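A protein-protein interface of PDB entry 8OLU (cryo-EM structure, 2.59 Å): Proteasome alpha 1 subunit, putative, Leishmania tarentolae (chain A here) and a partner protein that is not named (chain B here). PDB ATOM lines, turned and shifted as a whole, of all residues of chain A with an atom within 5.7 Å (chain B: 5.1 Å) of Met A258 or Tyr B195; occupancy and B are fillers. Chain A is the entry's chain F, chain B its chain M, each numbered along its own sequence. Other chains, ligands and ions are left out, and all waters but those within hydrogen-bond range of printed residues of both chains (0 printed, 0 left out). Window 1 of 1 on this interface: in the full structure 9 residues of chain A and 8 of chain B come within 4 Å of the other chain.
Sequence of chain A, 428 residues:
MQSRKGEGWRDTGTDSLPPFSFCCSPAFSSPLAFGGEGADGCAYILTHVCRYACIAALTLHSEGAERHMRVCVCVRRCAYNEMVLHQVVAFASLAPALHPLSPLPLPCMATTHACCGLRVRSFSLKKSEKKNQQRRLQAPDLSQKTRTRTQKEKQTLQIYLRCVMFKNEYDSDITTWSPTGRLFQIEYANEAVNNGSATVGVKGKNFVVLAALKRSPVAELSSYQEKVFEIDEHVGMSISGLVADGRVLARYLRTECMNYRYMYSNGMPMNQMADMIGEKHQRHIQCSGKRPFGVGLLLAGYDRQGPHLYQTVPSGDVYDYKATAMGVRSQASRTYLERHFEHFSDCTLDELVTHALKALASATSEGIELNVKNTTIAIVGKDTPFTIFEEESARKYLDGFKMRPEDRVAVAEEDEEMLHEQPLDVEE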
ATOM      1  N   ASP A 232      -3.788 -21.156  20.452  1.00  0.00           N
ATOM      2  CA  ASP A 232      -4.417 -21.247  21.749  1.00  0.00           C
ATOM      3  C   ASP A 232      -4.725 -22.717  21.909  1.00  0.00           C
ATOM      4  O   ASP A 232      -4.318 -23.501  21.093  1.00  0.00           O
ATOM      5  CB  ASP A 232      -5.596 -20.278  21.831  1.00  0.00           C
ATOM      6  CG  ASP A 232      -6.123 -20.099  23.258  1.00  0.00           C
ATOM      7  OD1 ASP A 232      -7.334 -19.736  23.451  1.00  0.00           O
ATOM      8  OD2 ASP A 232      -5.320 -20.322  24.189  1.00  0.00           O
ATOM      9  N   LEU A 253      -2.210 -13.459  16.131  1.00  0.00           N
ATOM     10  CA  LEU A 253      -3.282 -14.344  16.487  1.00  0.00           C
ATOM     11  C   LEU A 253      -3.150 -14.729  17.926  1.00  0.00           C
ATOM     12  O   LEU A 253      -4.133 -14.731  18.625  1.00  0.00           O
ATOM     13  CB  LEU A 253      -3.264 -15.599  15.661  1.00  0.00           C
ATOM     14  CG  LEU A 253      -3.676 -15.346  14.216  1.00  0.00           C
ATOM     15  CD1 LEU A 253      -3.495 -16.593  13.342  1.00  0.00           C
ATOM     16  CD2 LEU A 253      -5.124 -14.842  14.174  1.00  0.00           C
ATOM     17  N   ARG A 254      -1.968 -15.052  18.384  1.00  0.00           N
ATOM     18  CA  ARG A 254      -1.876 -15.465  19.770  1.00  0.00           C
ATOM     19  C   ARG A 254      -2.443 -14.401  20.668  1.00  0.00           C
ATOM     20  O   ARG A 254      -3.115 -14.692  21.617  1.00  0.00           O
ATOM     21  CB  ARG A 254      -0.428 -15.633  20.190  1.00  0.00           C
ATOM     22  CG  ARG A 254       0.015 -17.032  19.861  1.00  0.00           C
ATOM     23  CD  ARG A 254       1.439 -17.093  19.466  1.00  0.00           C
ATOM     24  NE  ARG A 254       1.857 -18.455  19.444  1.00  0.00           N
ATOM     25  CZ  ARG A 254       3.072 -18.799  19.150  1.00  0.00           C
ATOM     26  NH1 ARG A 254       4.012 -17.894  18.977  1.00  0.00           N
ATOM     27  NH2 ARG A 254       3.243 -20.073  18.918  1.00  0.00           N
ATOM     28  N   THR A 255      -2.057 -13.173  20.405  1.00  0.00           N
ATOM     29  CA  THR A 255      -2.454 -12.093  21.251  1.00  0.00           C
ATOM     30  C   THR A 255      -3.956 -11.868  21.191  1.00  0.00           C
ATOM     31  O   THR A 255      -4.559 -11.606  22.222  1.00  0.00           O
ATOM     32  CB  THR A 255      -1.788 -10.811  20.787  1.00  0.00           C
ATOM     33  OG1 THR A 255      -0.384 -11.037  20.827  1.00  0.00           O
ATOM     34  CG2 THR A 255      -2.173  -9.660  21.672  1.00  0.00           C
ATOM     35  N   GLU A 256      -4.550 -11.955  20.000  1.00  0.00           N
ATOM     36  CA  GLU A 256      -5.971 -11.755  19.910  1.00  0.00           C
ATOM     37  C   GLU A 256      -6.730 -12.874  20.600  1.00  0.00           C
ATOM     38  O   GLU A 256      -7.697 -12.603  21.334  1.00  0.00           O
ATOM     39  CB  GLU A 256      -6.437 -11.587  18.488  1.00  0.00           C
ATOM     40  CG  GLU A 256      -6.120 -10.200  17.897  1.00  0.00           C
ATOM     41  CD  GLU A 256      -6.299  -8.920  18.721  1.00  0.00           C
ATOM     42  OE1 GLU A 256      -7.424  -8.698  19.333  1.00  0.00           O
ATOM     43  OE2 GLU A 256      -5.288  -8.098  18.752  1.00  0.00           O
ATOM     44  N   CYS A 257      -6.248 -14.092  20.478  1.00  0.00           N
ATOM     45  CA  CYS A 257      -6.818 -15.160  21.234  1.00  0.00           C
ATOM     46  C   CYS A 257      -6.640 -15.037  22.720  1.00  0.00           C
ATOM     47  O   CYS A 257      -7.450 -15.545  23.461  1.00  0.00           O
ATOM     48  CB  CYS A 257      -6.227 -16.487  20.869  1.00  0.00           C
ATOM     49  SG  CYS A 257      -6.868 -16.974  19.254  1.00  0.00           S
ATOM     50  N   MET A 258      -5.575 -14.491  23.217  1.00  0.00           N
ATOM     51  CA  MET A 258      -5.533 -14.340  24.653  1.00  0.00           C
ATOM     52  C   MET A 258      -6.472 -13.214  25.056  1.00  0.00           C
ATOM     53  O   MET A 258      -7.078 -13.350  26.085  1.00  0.00           O
ATOM     54  CB  MET A 258      -4.127 -13.985  25.117  1.00  0.00           C
ATOM     55  CG  MET A 258      -3.130 -15.112  24.955  1.00  0.00           C
ATOM     56  SD  MET A 258      -1.533 -14.528  25.517  1.00  0.00           S
ATOM     57  CE  MET A 258      -0.351 -15.512  24.592  1.00  0.00           C
ATOM     58  N   ASN A 259      -6.558 -12.108  24.307  1.00  0.00           N
ATOM     59  CA  ASN A 259      -7.467 -11.086  24.726  1.00  0.00           C
ATOM     60  C   ASN A 259      -8.864 -11.680  24.783  1.00  0.00           C
ATOM     61  O   ASN A 259      -9.599 -11.522  25.768  1.00  0.00           O
ATOM     62  CB  ASN A 259      -7.524  -9.838  23.865  1.00  0.00           C
ATOM     63  CG  ASN A 259      -6.153  -9.206  23.638  1.00  0.00           C
ATOM     64  OD1 ASN A 259      -5.214  -9.389  24.436  1.00  0.00           O
ATOM     65  ND2 ASN A 259      -6.020  -8.479  22.519  1.00  0.00           N
ATOM     66  N   TYR A 260      -9.205 -12.450  23.752  1.00  0.00           N
ATOM     67  CA  TYR A 260     -10.548 -12.949  23.725  1.00  0.00           C
ATOM     68  C   TYR A 260     -10.750 -13.877  24.879  1.00  0.00           C
ATOM     69  O   TYR A 260     -11.774 -13.870  25.477  1.00  0.00           O
ATOM     70  CB  TYR A 260     -10.808 -13.739  22.473  1.00  0.00           C
ATOM     71  CG  TYR A 260     -12.215 -14.163  22.312  1.00  0.00           C
ATOM     72  CD1 TYR A 260     -13.105 -13.457  21.544  1.00  0.00           C
ATOM     73  CD2 TYR A 260     -12.653 -15.295  22.937  1.00  0.00           C
ATOM     74  CE1 TYR A 260     -14.429 -13.871  21.410  1.00  0.00           C
ATOM     75  CE2 TYR A 260     -13.953 -15.753  22.764  1.00  0.00           C
ATOM     76  CZ  TYR A 260     -14.857 -15.047  21.991  1.00  0.00           C
ATOM     77  OH  TYR A 260     -16.113 -15.557  21.926  1.00  0.00           O
ATOM     78  N   ARG A 261      -9.803 -14.704  25.197  1.00  0.00           N
ATOM     79  CA  ARG A 261     -10.064 -15.659  26.245  1.00  0.00           C
ATOM     80  C   ARG A 261     -10.063 -14.992  27.576  1.00  0.00           C
ATOM     81  O   ARG A 261     -10.773 -15.404  28.425  1.00  0.00           O
ATOM     82  CB  ARG A 261      -8.947 -16.658  26.241  1.00  0.00           C
ATOM     83  CG  ARG A 261      -9.113 -17.715  27.289  1.00  0.00           C
ATOM     84  CD  ARG A 261      -8.162 -18.844  26.983  1.00  0.00           C
ATOM     85  NE  ARG A 261      -8.649 -19.477  25.794  1.00  0.00           N
ATOM     86  CZ  ARG A 261      -9.329 -20.602  25.853  1.00  0.00           C
ATOM     87  NH1 ARG A 261     -10.012 -20.937  26.948  1.00  0.00           N
ATOM     88  NH2 ARG A 261      -9.348 -21.362  24.769  1.00  0.00           N
ATOM     89  N   TYR A 262      -9.264 -13.964  27.740  1.00  0.00           N
ATOM     90  CA  TYR A 262      -9.349 -13.131  28.914  1.00  0.00           C
ATOM     91  C   TYR A 262     -10.742 -12.560  29.073  1.00  0.00           C
ATOM     92  O   TYR A 262     -11.245 -12.512  30.169  1.00  0.00           O
ATOM     93  CB  TYR A 262      -8.416 -11.939  28.793  1.00  0.00           C
ATOM     94  CG  TYR A 262      -8.506 -10.924  29.874  1.00  0.00           C
ATOM     95  CD1 TYR A 262      -8.084 -11.219  31.149  1.00  0.00           C
ATOM     96  CD2 TYR A 262      -9.035  -9.672  29.632  1.00  0.00           C
ATOM     97  CE1 TYR A 262      -8.228 -10.273  32.174  1.00  0.00           C
ATOM     98  CE2 TYR A 262      -9.181  -8.705  30.629  1.00  0.00           C
ATOM     99  CZ  TYR A 262      -8.745  -9.003  31.899  1.00  0.00           C
ATOM    100  OH  TYR A 262      -8.808  -8.107  32.879  1.00  0.00           O
ATOM    101  N   MET A 263     -11.322 -12.026  28.018  1.00  0.00           N
ATOM    102  CA  MET A 263     -12.577 -11.344  28.173  1.00  0.00           C
ATOM    103  C   MET A 263     -13.677 -12.342  28.368  1.00  0.00           C
ATOM    104  O   MET A 263     -14.440 -12.190  29.286  1.00  0.00           O
ATOM    105  CB  MET A 263     -12.907 -10.500  26.956  1.00  0.00           C
ATOM    106  CG  MET A 263     -12.011  -9.288  26.881  1.00  0.00           C
ATOM    107  SD  MET A 263     -12.208  -8.110  28.254  1.00  0.00           S
ATOM    108  CE  MET A 263     -13.924  -7.802  27.873  1.00  0.00           C
ATOM    109  N   GLN B 191      -4.821 -13.801  35.806  1.00  0.00           N
ATOM    110  CA  GLN B 191      -4.865 -13.867  34.355  1.00  0.00           C
ATOM    111  C   GLN B 191      -3.624 -13.256  33.732  1.00  0.00           C
ATOM    112  O   GLN B 191      -3.080 -13.764  32.812  1.00  0.00           O
ATOM    113  CB  GLN B 191      -6.078 -13.118  33.817  1.00  0.00           C
ATOM    114  CG  GLN B 191      -7.412 -13.786  34.088  1.00  0.00           C
ATOM    115  CD  GLN B 191      -7.506 -15.189  33.574  1.00  0.00           C
ATOM    116  OE1 GLN B 191      -7.515 -15.405  32.373  1.00  0.00           O
ATOM    117  NE2 GLN B 191      -7.709 -16.139  34.441  1.00  0.00           N
ATOM    118  N   MET B 192      -3.191 -12.147  34.226  1.00  0.00           N
ATOM    119  CA  MET B 192      -1.956 -11.562  33.792  1.00  0.00           C
ATOM    120  C   MET B 192      -0.798 -12.548  33.849  1.00  0.00           C
ATOM    121  O   MET B 192       0.049 -12.548  32.981  1.00  0.00           O
ATOM    122  CB  MET B 192      -1.635 -10.383  34.696  1.00  0.00           C
ATOM    123  CG  MET B 192      -2.544  -9.218  34.433  1.00  0.00           C
ATOM    124  SD  MET B 192      -2.731  -8.777  32.707  1.00  0.00           S
ATOM    125  CE  MET B 192      -4.153  -9.724  32.094  1.00  0.00           C
ATOM    126  N   LEU B 193      -0.731 -13.349  34.882  1.00  0.00           N
ATOM    127  CA  LEU B 193       0.333 -14.298  34.992  1.00  0.00           C
ATOM    128  C   LEU B 193       0.120 -15.441  34.052  1.00  0.00           C
ATOM    129  O   LEU B 193       1.033 -16.076  33.647  1.00  0.00           O
ATOM    130  CB  LEU B 193       0.313 -14.873  36.398  1.00  0.00           C
ATOM    131  CG  LEU B 193       1.221 -14.124  37.348  1.00  0.00           C
ATOM    132  CD1 LEU B 193       1.043 -14.639  38.729  1.00  0.00           C
ATOM    133  CD2 LEU B 193       2.660 -14.348  36.986  1.00  0.00           C
ATOM    134  N   LYS B 194      -1.102 -15.861  33.949  1.00  0.00           N
ATOM    135  CA  LYS B 194      -1.398 -16.964  33.083  1.00  0.00           C
ATOM    136  C   LYS B 194      -0.989 -16.634  31.659  1.00  0.00           C
ATOM    137  O   LYS B 194      -0.570 -17.532  30.962  1.00  0.00           O
ATOM    138  CB  LYS B 194      -2.881 -17.273  33.184  1.00  0.00           C
ATOM    139  CG  LYS B 194      -3.419 -18.014  31.982  1.00  0.00           C
ATOM    140  CD  LYS B 194      -4.913 -18.037  31.927  1.00  0.00           C
ATOM    141  CE  LYS B 194      -5.376 -19.355  31.347  1.00  0.00           C
ATOM    142  NZ  LYS B 194      -6.238 -19.076  30.172  1.00  0.00           N
ATOM    143  N   TYR B 195      -1.061 -15.380  31.261  1.00  0.00           N
ATOM    144  CA  TYR B 195      -0.692 -15.028  29.911  1.00  0.00           C
ATOM    145  C   TYR B 195       0.808 -14.834  29.768  1.00  0.00           C
ATOM    146  O   TYR B 195       1.363 -15.166  28.735  1.00  0.00           O
ATOM    147  CB  TYR B 195      -1.558 -13.854  29.408  1.00  0.00           C
ATOM    148  CG  TYR B 195      -2.977 -14.348  29.168  1.00  0.00           C
ATOM    149  CD1 TYR B 195      -3.185 -15.473  28.349  1.00  0.00           C
ATOM    150  CD2 TYR B 195      -4.091 -13.847  29.874  1.00  0.00           C
ATOM    151  CE1 TYR B 195      -4.441 -16.053  28.207  1.00  0.00           C
ATOM    152  CE2 TYR B 195      -5.357 -14.427  29.747  1.00  0.00           C
ATOM    153  CZ  TYR B 195      -5.533 -15.496  28.859  1.00  0.00           C
ATOM    154  OH  TYR B 195      -6.732 -16.134  28.618  1.00  0.00           O
ATOM    155  N   ARG B 196       1.487 -14.282  30.777  1.00  0.00           N
ATOM    156  CA  ARG B 196       2.934 -14.267  30.767  1.00  0.00           C
ATOM    157  C   ARG B 196       3.471 -15.671  30.700  1.00  0.00           C
ATOM    158  O   ARG B 196       4.469 -15.916  30.058  1.00  0.00           O
ATOM    159  CB  ARG B 196       3.495 -13.525  31.962  1.00  0.00           C
ATOM    160  CG  ARG B 196       3.190 -12.035  31.920  1.00  0.00           C
ATOM    161  CD  ARG B 196       3.798 -11.282  30.770  1.00  0.00           C
ATOM    162  NE  ARG B 196       5.256 -11.360  30.951  1.00  0.00           N
ATOM    163  CZ  ARG B 196       6.008 -10.479  31.638  1.00  0.00           C
ATOM    164  NH1 ARG B 196       7.330 -10.593  31.635  1.00  0.00           N
ATOM    165  NH2 ARG B 196       5.409  -9.490  32.300  1.00  0.00           N
ATOM    166  N   VAL B 197       2.795 -16.614  31.280  1.00  0.00           N
ATOM    167  CA  VAL B 197       3.257 -17.962  31.225  1.00  0.00           C
ATOM    168  C   VAL B 197       2.978 -18.524  29.851  1.00  0.00           C
ATOM    169  O   VAL B 197       3.784 -19.279  29.356  1.00  0.00           O
ATOM    170  CB  VAL B 197       2.609 -18.774  32.341  1.00  0.00           C
ATOM    171  CG1 VAL B 197       2.840 -20.265  32.224  1.00  0.00           C
ATOM    172  CG2 VAL B 197       3.105 -18.335  33.680  1.00  0.00           C
ATOM    173  N   LYS B 198       1.865 -18.226  29.213  1.00  0.00           N
ATOM    174  CA  LYS B 198       1.692 -18.649  27.828  1.00  0.00           C
ATOM    175  C   LYS B 198       2.735 -18.004  26.924  1.00  0.00           C
ATOM    176  O   LYS B 198       3.386 -18.650  26.154  1.00  0.00           O
ATOM    177  CB  LYS B 198       0.284 -18.358  27.299  1.00  0.00           C
ATOM    178  CG  LYS B 198      -0.457 -19.646  26.970  1.00  0.00           C
ATOM    179  CD  LYS B 198      -1.688 -19.580  26.084  1.00  0.00           C
ATOM    180  CE  LYS B 198      -2.975 -19.480  26.875  1.00  0.00           C
ATOM    181  NZ  LYS B 198      -4.104 -19.057  26.003  1.00  0.00           N
ATOM    182  N   TRP B 199       2.981 -16.727  27.024  1.00  0.00           N
ATOM    183  CA  TRP B 199       4.043 -16.145  26.234  1.00  0.00           C
ATOM    184  C   TRP B 199       5.337 -16.862  26.473  1.00  0.00           C
ATOM    185  O   TRP B 199       6.096 -17.083  25.575  1.00  0.00           O
ATOM    186  CB  TRP B 199       4.233 -14.658  26.500  1.00  0.00           C
ATOM    187  CG  TRP B 199       3.194 -13.883  25.780  1.00  0.00           C
ATOM    188  CD1 TRP B 199       2.177 -13.161  26.330  1.00  0.00           C
ATOM    189  CD2 TRP B 199       2.922 -13.946  24.374  1.00  0.00           C
ATOM    190  NE1 TRP B 199       1.339 -12.698  25.339  1.00  0.00           N
ATOM    191  CE2 TRP B 199       1.774 -13.177  24.139  1.00  0.00           C
ATOM    192  CE3 TRP B 199       3.546 -14.582  23.308  1.00  0.00           C
ATOM    193  CZ2 TRP B 199       1.274 -12.960  22.876  1.00  0.00           C
ATOM    194  CZ3 TRP B 199       3.031 -14.414  22.046  1.00  0.00           C
ATOM    195  CH2 TRP B 199       1.930 -13.577  21.838  1.00  0.00           C
ATOM    196  N   TYR B 200       5.634 -17.176  27.692  1.00  0.00           N
ATOM    197  CA  TYR B 200       6.905 -17.779  27.966  1.00  0.00           C
ATOM    198  C   TYR B 200       6.947 -19.085  27.264  1.00  0.00           C
ATOM    199  O   TYR B 200       7.958 -19.348  26.688  1.00  0.00           O
ATOM    200  CB  TYR B 200       7.068 -17.981  29.461  1.00  0.00           C
ATOM    201  CG  TYR B 200       8.346 -18.623  29.876  1.00  0.00           C
ATOM    202  CD1 TYR B 200       8.593 -19.959  29.659  1.00  0.00           C
ATOM    203  CD2 TYR B 200       9.342 -17.850  30.445  1.00  0.00           C
ATOM    204  CE1 TYR B 200       9.793 -20.530  30.047  1.00  0.00           C
ATOM    205  CE2 TYR B 200      10.533 -18.412  30.855  1.00  0.00           C
ATOM    206  CZ  TYR B 200      10.751 -19.748  30.642  1.00  0.00           C
ATOM    207  OH  TYR B 200      11.937 -20.218  31.088  1.00  0.00           O
ATOM    208  N   TYR B 202       5.575 -19.971  24.567  1.00  0.00           N
ATOM    209  CA  TYR B 202       5.699 -19.878  23.119  1.00  0.00           C
ATOM    210  C   TYR B 202       7.096 -19.419  22.730  1.00  0.00           C
ATOM    211  O   TYR B 202       7.732 -19.997  21.880  1.00  0.00           O
ATOM    212  CB  TYR B 202       4.717 -18.880  22.510  1.00  0.00           C
ATOM    213  CG  TYR B 202       3.255 -19.244  22.592  1.00  0.00           C
ATOM    214  CD1 TYR B 202       2.844 -20.537  22.382  1.00  0.00           C
ATOM    215  CD2 TYR B 202       2.280 -18.271  22.842  1.00  0.00           C
ATOM    216  CE1 TYR B 202       1.495 -20.881  22.436  1.00  0.00           C
ATOM    217  CE2 TYR B 202       0.933 -18.585  22.914  1.00  0.00           C
ATOM    218  CZ  TYR B 202       0.545 -19.905  22.716  1.00  0.00           C
ATOM    219  OH  TYR B 202      -0.769 -20.321  22.755  1.00  0.00           O
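The side-chain hydroxyl (OH) of Tyr B195 sits at hydrogen-bond distance from the backbone NH (N) of Tyr A262 (3.4 Å). The side-chain amino group (NZ) of Lys B198 lies within salt-bridge range of the side-chain carboxylate (OD2) of Asp A232 (2.5 Å). NE1 of Trp B199 lies close to SD of Met A258, 3.4 Å away.
Hydrophobic or aromatic side chains of chain A that line the printed part of chain B: Met A258 and Tyr A262. Of the 11 printed residues of chain B, 6 touch a printed residue of chain A.
The side-chain amino group (NZ) of Lys B194 sits at hydrogen-bond distance from the side-chain hydroxyl (OH) of Tyr B195 (3.4 Å). The side-chain carboxylate (OD1) of Asp A232 lies within salt-bridge range of the guanidinium group (NE) of Arg A261, at 2.7 Å. The backbone carbonyl oxygen (O) of Thr A255 sits close to the side-chain amide oxygen (OD1) of Asn A259 (3.2 Å).
Asp A232 touches Tyr B202 (N to OH, 3.9 Å). Trp B199 touches Arg A254. Tyr B202 touches Arg A254 (CD2 to NE, 3.4 Å). OG1 of Thr A255 touches CZ2 of Trp B199, 3.3 Å away. Met A258 touches Tyr B195. Met A258 touches Lys B198 (CE to CB, 3.98 Å). Met A258 touches Tyr B202. Lys B194 touches Arg A261. CG of Arg A261 touches OH of Tyr B195, at 3.2 Å. CB of Gln B191 touches CD1 of Tyr A262 (3.8 Å).
Of the printed residues of chain B, Asp A232 touches Lys B198 (2.5 Å) and Tyr B202 (3.9 Å). Of the printed residues of chain B, Met A258 touches Tyr B195, Lys B198, Trp B199 and Tyr B202. Printed residues of chain A within 4 Å of Gln B191: Tyr A262 (3.8 Å). Of chain A, only Met A258, Arg A261 and Tyr A262 come within 4 Å of Tyr B195. Of the printed residues of chain A, Lys B198 touches Asp A232 and Met A258. Printed residues of chain A within 4 Å of Trp B199: Arg A254, Thr A255 and Met A258. The nearest printed residue of chain B that does not touch Met A258 is Arg B196 (6.1 Å). The nearest residue of chain A that does not touch Tyr B195 is Cys A257 (5.2 Å).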
